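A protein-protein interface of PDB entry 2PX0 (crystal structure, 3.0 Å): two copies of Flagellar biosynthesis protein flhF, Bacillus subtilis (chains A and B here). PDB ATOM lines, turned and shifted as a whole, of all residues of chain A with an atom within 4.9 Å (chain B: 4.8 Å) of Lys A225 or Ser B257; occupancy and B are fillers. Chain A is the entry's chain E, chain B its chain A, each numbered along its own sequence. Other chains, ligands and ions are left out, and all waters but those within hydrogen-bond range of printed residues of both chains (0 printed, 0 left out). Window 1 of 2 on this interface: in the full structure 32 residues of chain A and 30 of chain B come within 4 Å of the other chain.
O of Thr B223 touches O of Thr A223, 3.95 Å away.
O of Thr A223 touches CA of Ala B224 (3.5 Å).
Thr B223 touches Ala A224.
Ala A224 touches Lys B225 (O to CE, 3.7 Å).
Lys A225 touches Ala B224 (CG to O, 3.2 Å).
Lys A225 touches Lys B225 (CG to CA, 3.7 Å).
CG2 of Thr B223 touches OD2 of Asp A228, 3.2 Å away.
Thr A223 touches Ala B224, and with the chains exchanged Ala A224 touches Thr B223.
Thr A223 touches Lys B225, and with the chains exchanged Lys A225 touches Thr B223.
Ala A224 touches Lys B225, and with the chains exchanged Lys A225 touches Ala B224.
Lys B225 touches its own counterpart, Lys A225.
Positions printed for both chains: 223, 224, 225, 226 and 229.
Of the 14 pairs that touch across the chains among the printed residues, 8 have their exchanged pair printed and touching as well.
Of the printed residues of chain B, Lys A225 touches Ala B222, Thr B223, Ala B224, Lys B225, Thr B252, Ser B254 and Ser B257.
Printed residues of chain B within 4 Å of Asp A228: Thr B223 (3.2 Å) and Thr B252 (3.4 Å).
Met A229 touches none of the printed residues of chain B.
Of the printed residues of chain A, Ala B222 touches Lys A225 (3.0 Å).
Of the printed residues of chain A, Thr B252 touches Lys A225 (2.8 Å) and Asp A228 (3.4 Å).
Printed residues of chain A within 4 Å of Ser B254: Lys A225.
Ser B257 touches just one residue of chain A: Lys A225 (3.1 Å).
Ile B261 touches none of the printed residues of chain A.
The nearest printed residue of chain B that does not touch Lys A225 is Leu B255 (5.1 Å).
The nearest printed residue of chain A that does not touch Ser B254 is Asp A228 (4.7 Å).
The side-chain hydroxyl (OG1) of Thr B252 sits at hydrogen-bond distance from the side-chain amino group (NZ) of Lys A225.
The backbone carbonyl oxygen (O) of Ala B222 lies within hydrogen-bond range of the side-chain amino group (NZ) of Lys A225, at 3.0 Å.
The backbone carbonyl oxygen (O) of Thr B223 lies within hydrogen-bond range of the backbone NH (N) of Lys A225.
The backbone carbonyl oxygen of Ser B254 sits at hydrogen-bond distance from the side-chain amino group of Lys A225 (3.2 Å).
The side-chain hydroxyl (OG) of Ser B257 lies within hydrogen-bond range of the side-chain amino group (NZ) of Lys A225 (3.1 Å).
The backbone carbonyl oxygen (O) of Thr A223 sits close to the backbone NH (N) of Lys B225 (3.3 Å).
OG1 of Thr B252 sits at hydrogen-bond distance from OD1 of Asp A228 (3.4 Å).
The side-chain hydroxyl of Ser B254 sits at hydrogen-bond distance from the backbone NH of Gly B256, 3.0 Å away.
The backbone NH (N) of Gly B53 lies within hydrogen-bond range of the side-chain hydroxyl (OG) of Ser B254, at 2.7 Å.
N of Ser B257 lies close to ND2 of Asn B260, at 3.3 Å.
The side-chain hydroxyl of Thr B252 sits at hydrogen-bond distance from the backbone carbonyl oxygen of Ala B222 (3.0 Å).
The side-chain hydroxyl (OG1) of Thr B252 is in hydrogen-bond range of the backbone carbonyl oxygen (O) of Ser B254 (3.0 Å).
Hydrophobic or aromatic side chains of chain B within 4 Å of the printed part of chain A: Ala B224.
Along chain B the printed residues that touch a printed residue of chain A span positions 222 to 257.
Of the 7 printed residues of chain A, 4 touch a printed residue of chain B.
Printed residues of chain A that touch a printed residue of chain B: Thr A223, Ala A224, Lys A225 and Asp A228.
Hydrophobic or aromatic side chains of chain A that line the printed part of chain B: Ala A224.
Among the printed residues, 14 pairs touch across the chains.
Among the printed residues, no Asp or Glu carboxylate lies within 4 Å of a Lys or Arg side-chain nitrogen of the other chain.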
ATOM      1  N   THR A 223      10.340 -12.646 -10.359  1.00  0.00           N
ATOM      2  CA  THR A 223       9.448 -12.423  -9.219  1.00  0.00           C
ATOM      3  C   THR A 223       9.191 -13.687  -8.384  1.00  0.00           C
ATOM      4  O   THR A 223       8.927 -13.602  -7.190  1.00  0.00           O
ATOM      5  CB  THR A 223       8.089 -11.860  -9.716  1.00  0.00           C
ATOM      6  OG1 THR A 223       8.271 -10.517 -10.166  1.00  0.00           O
ATOM      7  CG2 THR A 223       7.051 -11.863  -8.612  1.00  0.00           C
ATOM      8  N   ALA A 224       9.274 -14.849  -9.025  1.00  0.00           N
ATOM      9  CA  ALA A 224       9.039 -16.134  -8.374  1.00  0.00           C
ATOM     10  C   ALA A 224      10.056 -16.514  -7.295  1.00  0.00           C
ATOM     11  O   ALA A 224      11.243 -16.190  -7.381  1.00  0.00           O
ATOM     12  CB  ALA A 224       8.978 -17.231  -9.422  1.00  0.00           C
ATOM     13  N   LYS A 225       9.569 -17.224  -6.285  1.00  0.00           N
ATOM     14  CA  LYS A 225      10.390 -17.673  -5.181  1.00  0.00           C
ATOM     15  C   LYS A 225      11.272 -18.783  -5.699  1.00  0.00           C
ATOM     16  O   LYS A 225      10.850 -19.556  -6.541  1.00  0.00           O
ATOM     17  CB  LYS A 225       9.495 -18.178  -4.053  1.00  0.00           C
ATOM     18  CG  LYS A 225       8.598 -17.094  -3.474  1.00  0.00           C
ATOM     19  CD  LYS A 225       7.716 -17.605  -2.341  1.00  0.00           C
ATOM     20  CE  LYS A 225       6.501 -18.352  -2.870  1.00  0.00           C
ATOM     21  NZ  LYS A 225       5.549 -18.701  -1.796  1.00  0.00           N
ATOM     22  N   TYR A 226      12.499 -18.863  -5.197  1.00  0.00           N
ATOM     23  CA  TYR A 226      13.438 -19.880  -5.643  1.00  0.00           C
ATOM     24  C   TYR A 226      12.894 -21.294  -5.500  1.00  0.00           C
ATOM     25  O   TYR A 226      12.875 -22.070  -6.464  1.00  0.00           O
ATOM     26  CB  TYR A 226      14.747 -19.764  -4.867  1.00  0.00           C
ATOM     27  CG  TYR A 226      15.685 -20.943  -5.057  1.00  0.00           C
ATOM     28  CD1 TYR A 226      16.170 -21.280  -6.326  1.00  0.00           C
ATOM     29  CD2 TYR A 226      16.058 -21.745  -3.974  1.00  0.00           C
ATOM     30  CE1 TYR A 226      17.003 -22.389  -6.513  1.00  0.00           C
ATOM     31  CE2 TYR A 226      16.887 -22.849  -4.152  1.00  0.00           C
ATOM     32  CZ  TYR A 226      17.354 -23.165  -5.424  1.00  0.00           C
ATOM     33  OH  TYR A 226      18.173 -24.251  -5.603  1.00  0.00           O
ATOM     34  N   GLU A 227      12.461 -21.628  -4.287  1.00  0.00           N
ATOM     35  CA  GLU A 227      11.934 -22.955  -3.992  1.00  0.00           C
ATOM     36  C   GLU A 227      10.891 -23.351  -5.042  1.00  0.00           C
ATOM     37  O   GLU A 227      10.827 -24.514  -5.467  1.00  0.00           O
ATOM     38  CB  GLU A 227      11.342 -22.967  -2.580  1.00  0.00           C
ATOM     39  CG  GLU A 227      11.511 -24.291  -1.823  1.00  0.00           C
ATOM     40  CD  GLU A 227      12.969 -24.661  -1.514  1.00  0.00           C
ATOM     41  OE1 GLU A 227      13.704 -23.820  -0.937  1.00  0.00           O
ATOM     42  OE2 GLU A 227      13.373 -25.805  -1.833  1.00  0.00           O
ATOM     43  N   ASP A 228      10.090 -22.385  -5.487  1.00  0.00           N
ATOM     44  CA  ASP A 228       9.081 -22.670  -6.501  1.00  0.00           C
ATOM     45  C   ASP A 228       9.744 -23.024  -7.810  1.00  0.00           C
ATOM     46  O   ASP A 228       9.591 -24.140  -8.293  1.00  0.00           O
ATOM     47  CB  ASP A 228       8.156 -21.477  -6.723  1.00  0.00           C
ATOM     48  CG  ASP A 228       7.240 -21.221  -5.547  1.00  0.00           C
ATOM     49  OD1 ASP A 228       7.078 -22.127  -4.695  1.00  0.00           O
ATOM     50  OD2 ASP A 228       6.675 -20.108  -5.491  1.00  0.00           O
ATOM     51  N   MET A 229      10.483 -22.072  -8.374  1.00  0.00           N
ATOM     52  CA  MET A 229      11.188 -22.271  -9.641  1.00  0.00           C
ATOM     53  C   MET A 229      11.984 -23.577  -9.688  1.00  0.00           C
ATOM     54  O   MET A 229      11.879 -24.339 -10.647  1.00  0.00           O
ATOM     55  CB  MET A 229      12.124 -21.090  -9.916  1.00  0.00           C
ATOM     56  CG  MET A 229      11.400 -19.755 -10.064  1.00  0.00           C
ATOM     57  SD  MET A 229      12.466 -18.358 -10.497  1.00  0.00           S
ATOM     58  CE  MET A 229      13.140 -17.888  -8.863  1.00  0.00           C
ATOM     59  N   GLY B  53       7.485 -20.864   5.004  1.00  0.00           N
ATOM     60  CA  GLY B  53       8.286 -19.743   4.548  1.00  0.00           C
ATOM     61  C   GLY B  53       8.469 -18.661   5.591  1.00  0.00           C
ATOM     62  O   GLY B  53       9.176 -17.682   5.347  1.00  0.00           O
ATOM     63  N   ALA B 222       0.590 -16.038  -4.893  1.00  0.00           N
ATOM     64  CA  ALA B 222       1.256 -16.867  -3.892  1.00  0.00           C
ATOM     65  C   ALA B 222       2.647 -17.334  -4.343  1.00  0.00           C
ATOM     66  O   ALA B 222       3.323 -18.103  -3.655  1.00  0.00           O
ATOM     67  CB  ALA B 222       0.370 -18.074  -3.563  1.00  0.00           C
ATOM     68  N   THR B 223       3.088 -16.856  -5.493  1.00  0.00           N
ATOM     69  CA  THR B 223       4.392 -17.264  -5.993  1.00  0.00           C
ATOM     70  C   THR B 223       5.480 -16.205  -5.773  1.00  0.00           C
ATOM     71  O   THR B 223       6.664 -16.517  -5.778  1.00  0.00           O
ATOM     72  CB  THR B 223       4.303 -17.623  -7.488  1.00  0.00           C
ATOM     73  OG1 THR B 223       3.223 -18.539  -7.691  1.00  0.00           O
ATOM     74  CG2 THR B 223       5.566 -18.297  -7.935  1.00  0.00           C
ATOM     75  N   ALA B 224       5.060 -14.960  -5.570  1.00  0.00           N
ATOM     76  CA  ALA B 224       5.968 -13.848  -5.328  1.00  0.00           C
ATOM     77  C   ALA B 224       6.818 -14.017  -4.071  1.00  0.00           C
ATOM     78  O   ALA B 224       6.466 -14.739  -3.146  1.00  0.00           O
ATOM     79  CB  ALA B 224       5.186 -12.576  -5.216  1.00  0.00           C
ATOM     80  N   LYS B 225       7.946 -13.331  -4.043  1.00  0.00           N
ATOM     81  CA  LYS B 225       8.817 -13.403  -2.900  1.00  0.00           C
ATOM     82  C   LYS B 225       8.196 -12.452  -1.889  1.00  0.00           C
ATOM     83  O   LYS B 225       7.511 -11.502  -2.263  1.00  0.00           O
ATOM     84  CB  LYS B 225      10.221 -12.934  -3.266  1.00  0.00           C
ATOM     85  CG  LYS B 225      10.758 -13.478  -4.571  1.00  0.00           C
ATOM     86  CD  LYS B 225      12.275 -13.348  -4.605  1.00  0.00           C
ATOM     87  CE  LYS B 225      12.827 -13.129  -6.002  1.00  0.00           C
ATOM     88  NZ  LYS B 225      12.577 -11.750  -6.464  1.00  0.00           N
ATOM     89  N   TYR B 226       8.426 -12.717  -0.612  1.00  0.00           N
ATOM     90  CA  TYR B 226       7.886 -11.873   0.440  1.00  0.00           C
ATOM     91  C   TYR B 226       8.379 -10.439   0.310  1.00  0.00           C
ATOM     92  O   TYR B 226       7.601  -9.486   0.410  1.00  0.00           O
ATOM     93  CB  TYR B 226       8.299 -12.406   1.820  1.00  0.00           C
ATOM     94  CG  TYR B 226       8.129 -11.384   2.931  1.00  0.00           C
ATOM     95  CD1 TYR B 226       6.859 -10.995   3.362  1.00  0.00           C
ATOM     96  CD2 TYR B 226       9.234 -10.769   3.510  1.00  0.00           C
ATOM     97  CE1 TYR B 226       6.695 -10.018   4.339  1.00  0.00           C
ATOM     98  CE2 TYR B 226       9.080  -9.793   4.482  1.00  0.00           C
ATOM     99  CZ  TYR B 226       7.808  -9.423   4.894  1.00  0.00           C
ATOM    100  OH  TYR B 226       7.644  -8.467   5.865  1.00  0.00           O
ATOM    101  N   MET B 229       6.536  -8.351  -2.214  1.00  0.00           N
ATOM    102  CA  MET B 229       5.195  -8.006  -1.745  1.00  0.00           C
ATOM    103  C   MET B 229       5.272  -7.032  -0.579  1.00  0.00           C
ATOM    104  O   MET B 229       4.437  -6.136  -0.454  1.00  0.00           O
ATOM    105  CB  MET B 229       4.444  -9.250  -1.288  1.00  0.00           C
ATOM    106  CG  MET B 229       4.135 -10.254  -2.367  1.00  0.00           C
ATOM    107  SD  MET B 229       3.209 -11.649  -1.644  1.00  0.00           S
ATOM    108  CE  MET B 229       4.552 -12.696  -1.036  1.00  0.00           C
ATOM    109  N   THR B 252       2.492 -22.759  -5.714  1.00  0.00           N
ATOM    110  CA  THR B 252       3.601 -22.436  -4.824  1.00  0.00           C
ATOM    111  C   THR B 252       3.985 -23.647  -3.984  1.00  0.00           C
ATOM    112  O   THR B 252       3.312 -24.662  -4.035  1.00  0.00           O
ATOM    113  CB  THR B 252       3.233 -21.235  -3.923  1.00  0.00           C
ATOM    114  OG1 THR B 252       4.350 -20.880  -3.100  1.00  0.00           O
ATOM    115  CG2 THR B 252       2.034 -21.556  -3.069  1.00  0.00           C
ATOM    116  N   SER B 254       5.370 -23.215  -0.474  1.00  0.00           N
ATOM    117  CA  SER B 254       5.112 -22.876   0.912  1.00  0.00           C
ATOM    118  C   SER B 254       4.205 -21.648   0.920  1.00  0.00           C
ATOM    119  O   SER B 254       4.019 -20.998  -0.102  1.00  0.00           O
ATOM    120  CB  SER B 254       6.431 -22.579   1.626  1.00  0.00           C
ATOM    121  OG  SER B 254       6.225 -21.823   2.808  1.00  0.00           O
ATOM    122  N   LEU B 255       3.624 -21.331   2.065  1.00  0.00           N
ATOM    123  CA  LEU B 255       2.744 -20.193   2.154  1.00  0.00           C
ATOM    124  C   LEU B 255       3.278 -19.200   3.172  1.00  0.00           C
ATOM    125  O   LEU B 255       2.609 -18.225   3.534  1.00  0.00           O
ATOM    126  CB  LEU B 255       1.346 -20.670   2.523  1.00  0.00           C
ATOM    127  CG  LEU B 255       0.513 -21.172   1.339  1.00  0.00           C
ATOM    128  CD1 LEU B 255      -0.708 -21.907   1.826  1.00  0.00           C
ATOM    129  CD2 LEU B 255       0.086 -19.987   0.494  1.00  0.00           C
ATOM    130  N   GLY B 256       4.504 -19.444   3.622  1.00  0.00           N
ATOM    131  CA  GLY B 256       5.110 -18.549   4.591  1.00  0.00           C
ATOM    132  C   GLY B 256       5.023 -17.088   4.168  1.00  0.00           C
ATOM    133  O   GLY B 256       4.544 -16.241   4.929  1.00  0.00           O
ATOM    134  N   SER B 257       5.476 -16.789   2.950  1.00  0.00           N
ATOM    135  CA  SER B 257       5.451 -15.426   2.450  1.00  0.00           C
ATOM    136  C   SER B 257       4.065 -14.782   2.574  1.00  0.00           C
ATOM    137  O   SER B 257       3.938 -13.603   2.944  1.00  0.00           O
ATOM    138  CB  SER B 257       5.920 -15.399   0.995  1.00  0.00           C
ATOM    139  OG  SER B 257       5.242 -16.355   0.206  1.00  0.00           O
ATOM    140  N   VAL B 258       3.021 -15.551   2.271  1.00  0.00           N
ATOM    141  CA  VAL B 258       1.670 -15.014   2.351  1.00  0.00           C
ATOM    142  C   VAL B 258       1.337 -14.716   3.820  1.00  0.00           C
ATOM    143  O   VAL B 258       0.607 -13.774   4.129  1.00  0.00           O
ATOM    144  CB  VAL B 258       0.642 -16.000   1.725  1.00  0.00           C
ATOM    145  CG1 VAL B 258      -0.717 -15.341   1.599  1.00  0.00           C
ATOM    146  CG2 VAL B 258       1.129 -16.437   0.359  1.00  0.00           C
ATOM    147  N   PHE B 259       1.878 -15.519   4.728  1.00  0.00           N
ATOM    148  CA  PHE B 259       1.663 -15.284   6.151  1.00  0.00           C
ATOM    149  C   PHE B 259       2.396 -13.992   6.511  1.00  0.00           C
ATOM    150  O   PHE B 259       1.799 -13.029   7.009  1.00  0.00           O
ATOM    151  CB  PHE B 259       2.224 -16.451   6.963  1.00  0.00           C
ATOM    152  CG  PHE B 259       2.081 -16.283   8.443  1.00  0.00           C
ATOM    153  CD1 PHE B 259       3.031 -15.582   9.164  1.00  0.00           C
ATOM    154  CD2 PHE B 259       0.999 -16.830   9.117  1.00  0.00           C
ATOM    155  CE1 PHE B 259       2.914 -15.428  10.543  1.00  0.00           C
ATOM    156  CE2 PHE B 259       0.874 -16.682  10.491  1.00  0.00           C
ATOM    157  CZ  PHE B 259       1.833 -15.979  11.208  1.00  0.00           C
ATOM    158  N   ASN B 260       3.698 -13.981   6.239  1.00  0.00           N
ATOM    159  CA  ASN B 260       4.523 -12.807   6.489  1.00  0.00           C
ATOM    160  C   ASN B 260       3.784 -11.504   6.137  1.00  0.00           C
ATOM    161  O   ASN B 260       3.794 -10.544   6.908  1.00  0.00           O
ATOM    162  CB  ASN B 260       5.805 -12.882   5.658  1.00  0.00           C
ATOM    163  CG  ASN B 260       6.700 -14.038   6.051  1.00  0.00           C
ATOM    164  OD1 ASN B 260       7.057 -14.207   7.225  1.00  0.00           O
ATOM    165  ND2 ASN B 260       7.088 -14.836   5.063  1.00  0.00           N
ATOM    166  N   ILE B 261       3.154 -11.482   4.964  1.00  0.00           N
ATOM    167  CA  ILE B 261       2.433 -10.307   4.494  1.00  0.00           C
ATOM    168  C   ILE B 261       1.211 -10.008   5.325  1.00  0.00           C
ATOM    169  O   ILE B 261       0.877  -8.840   5.573  1.00  0.00           O
ATOM    170  CB  ILE B 261       1.973 -10.463   3.029  1.00  0.00           C
ATOM    171  CG1 ILE B 261       3.162 -10.320   2.085  1.00  0.00           C
ATOM    172  CG2 ILE B 261       0.962  -9.405   2.688  1.00  0.00           C
ATOM    173  CD1 ILE B 261       3.868  -9.001   2.206  1.00  0.00           C
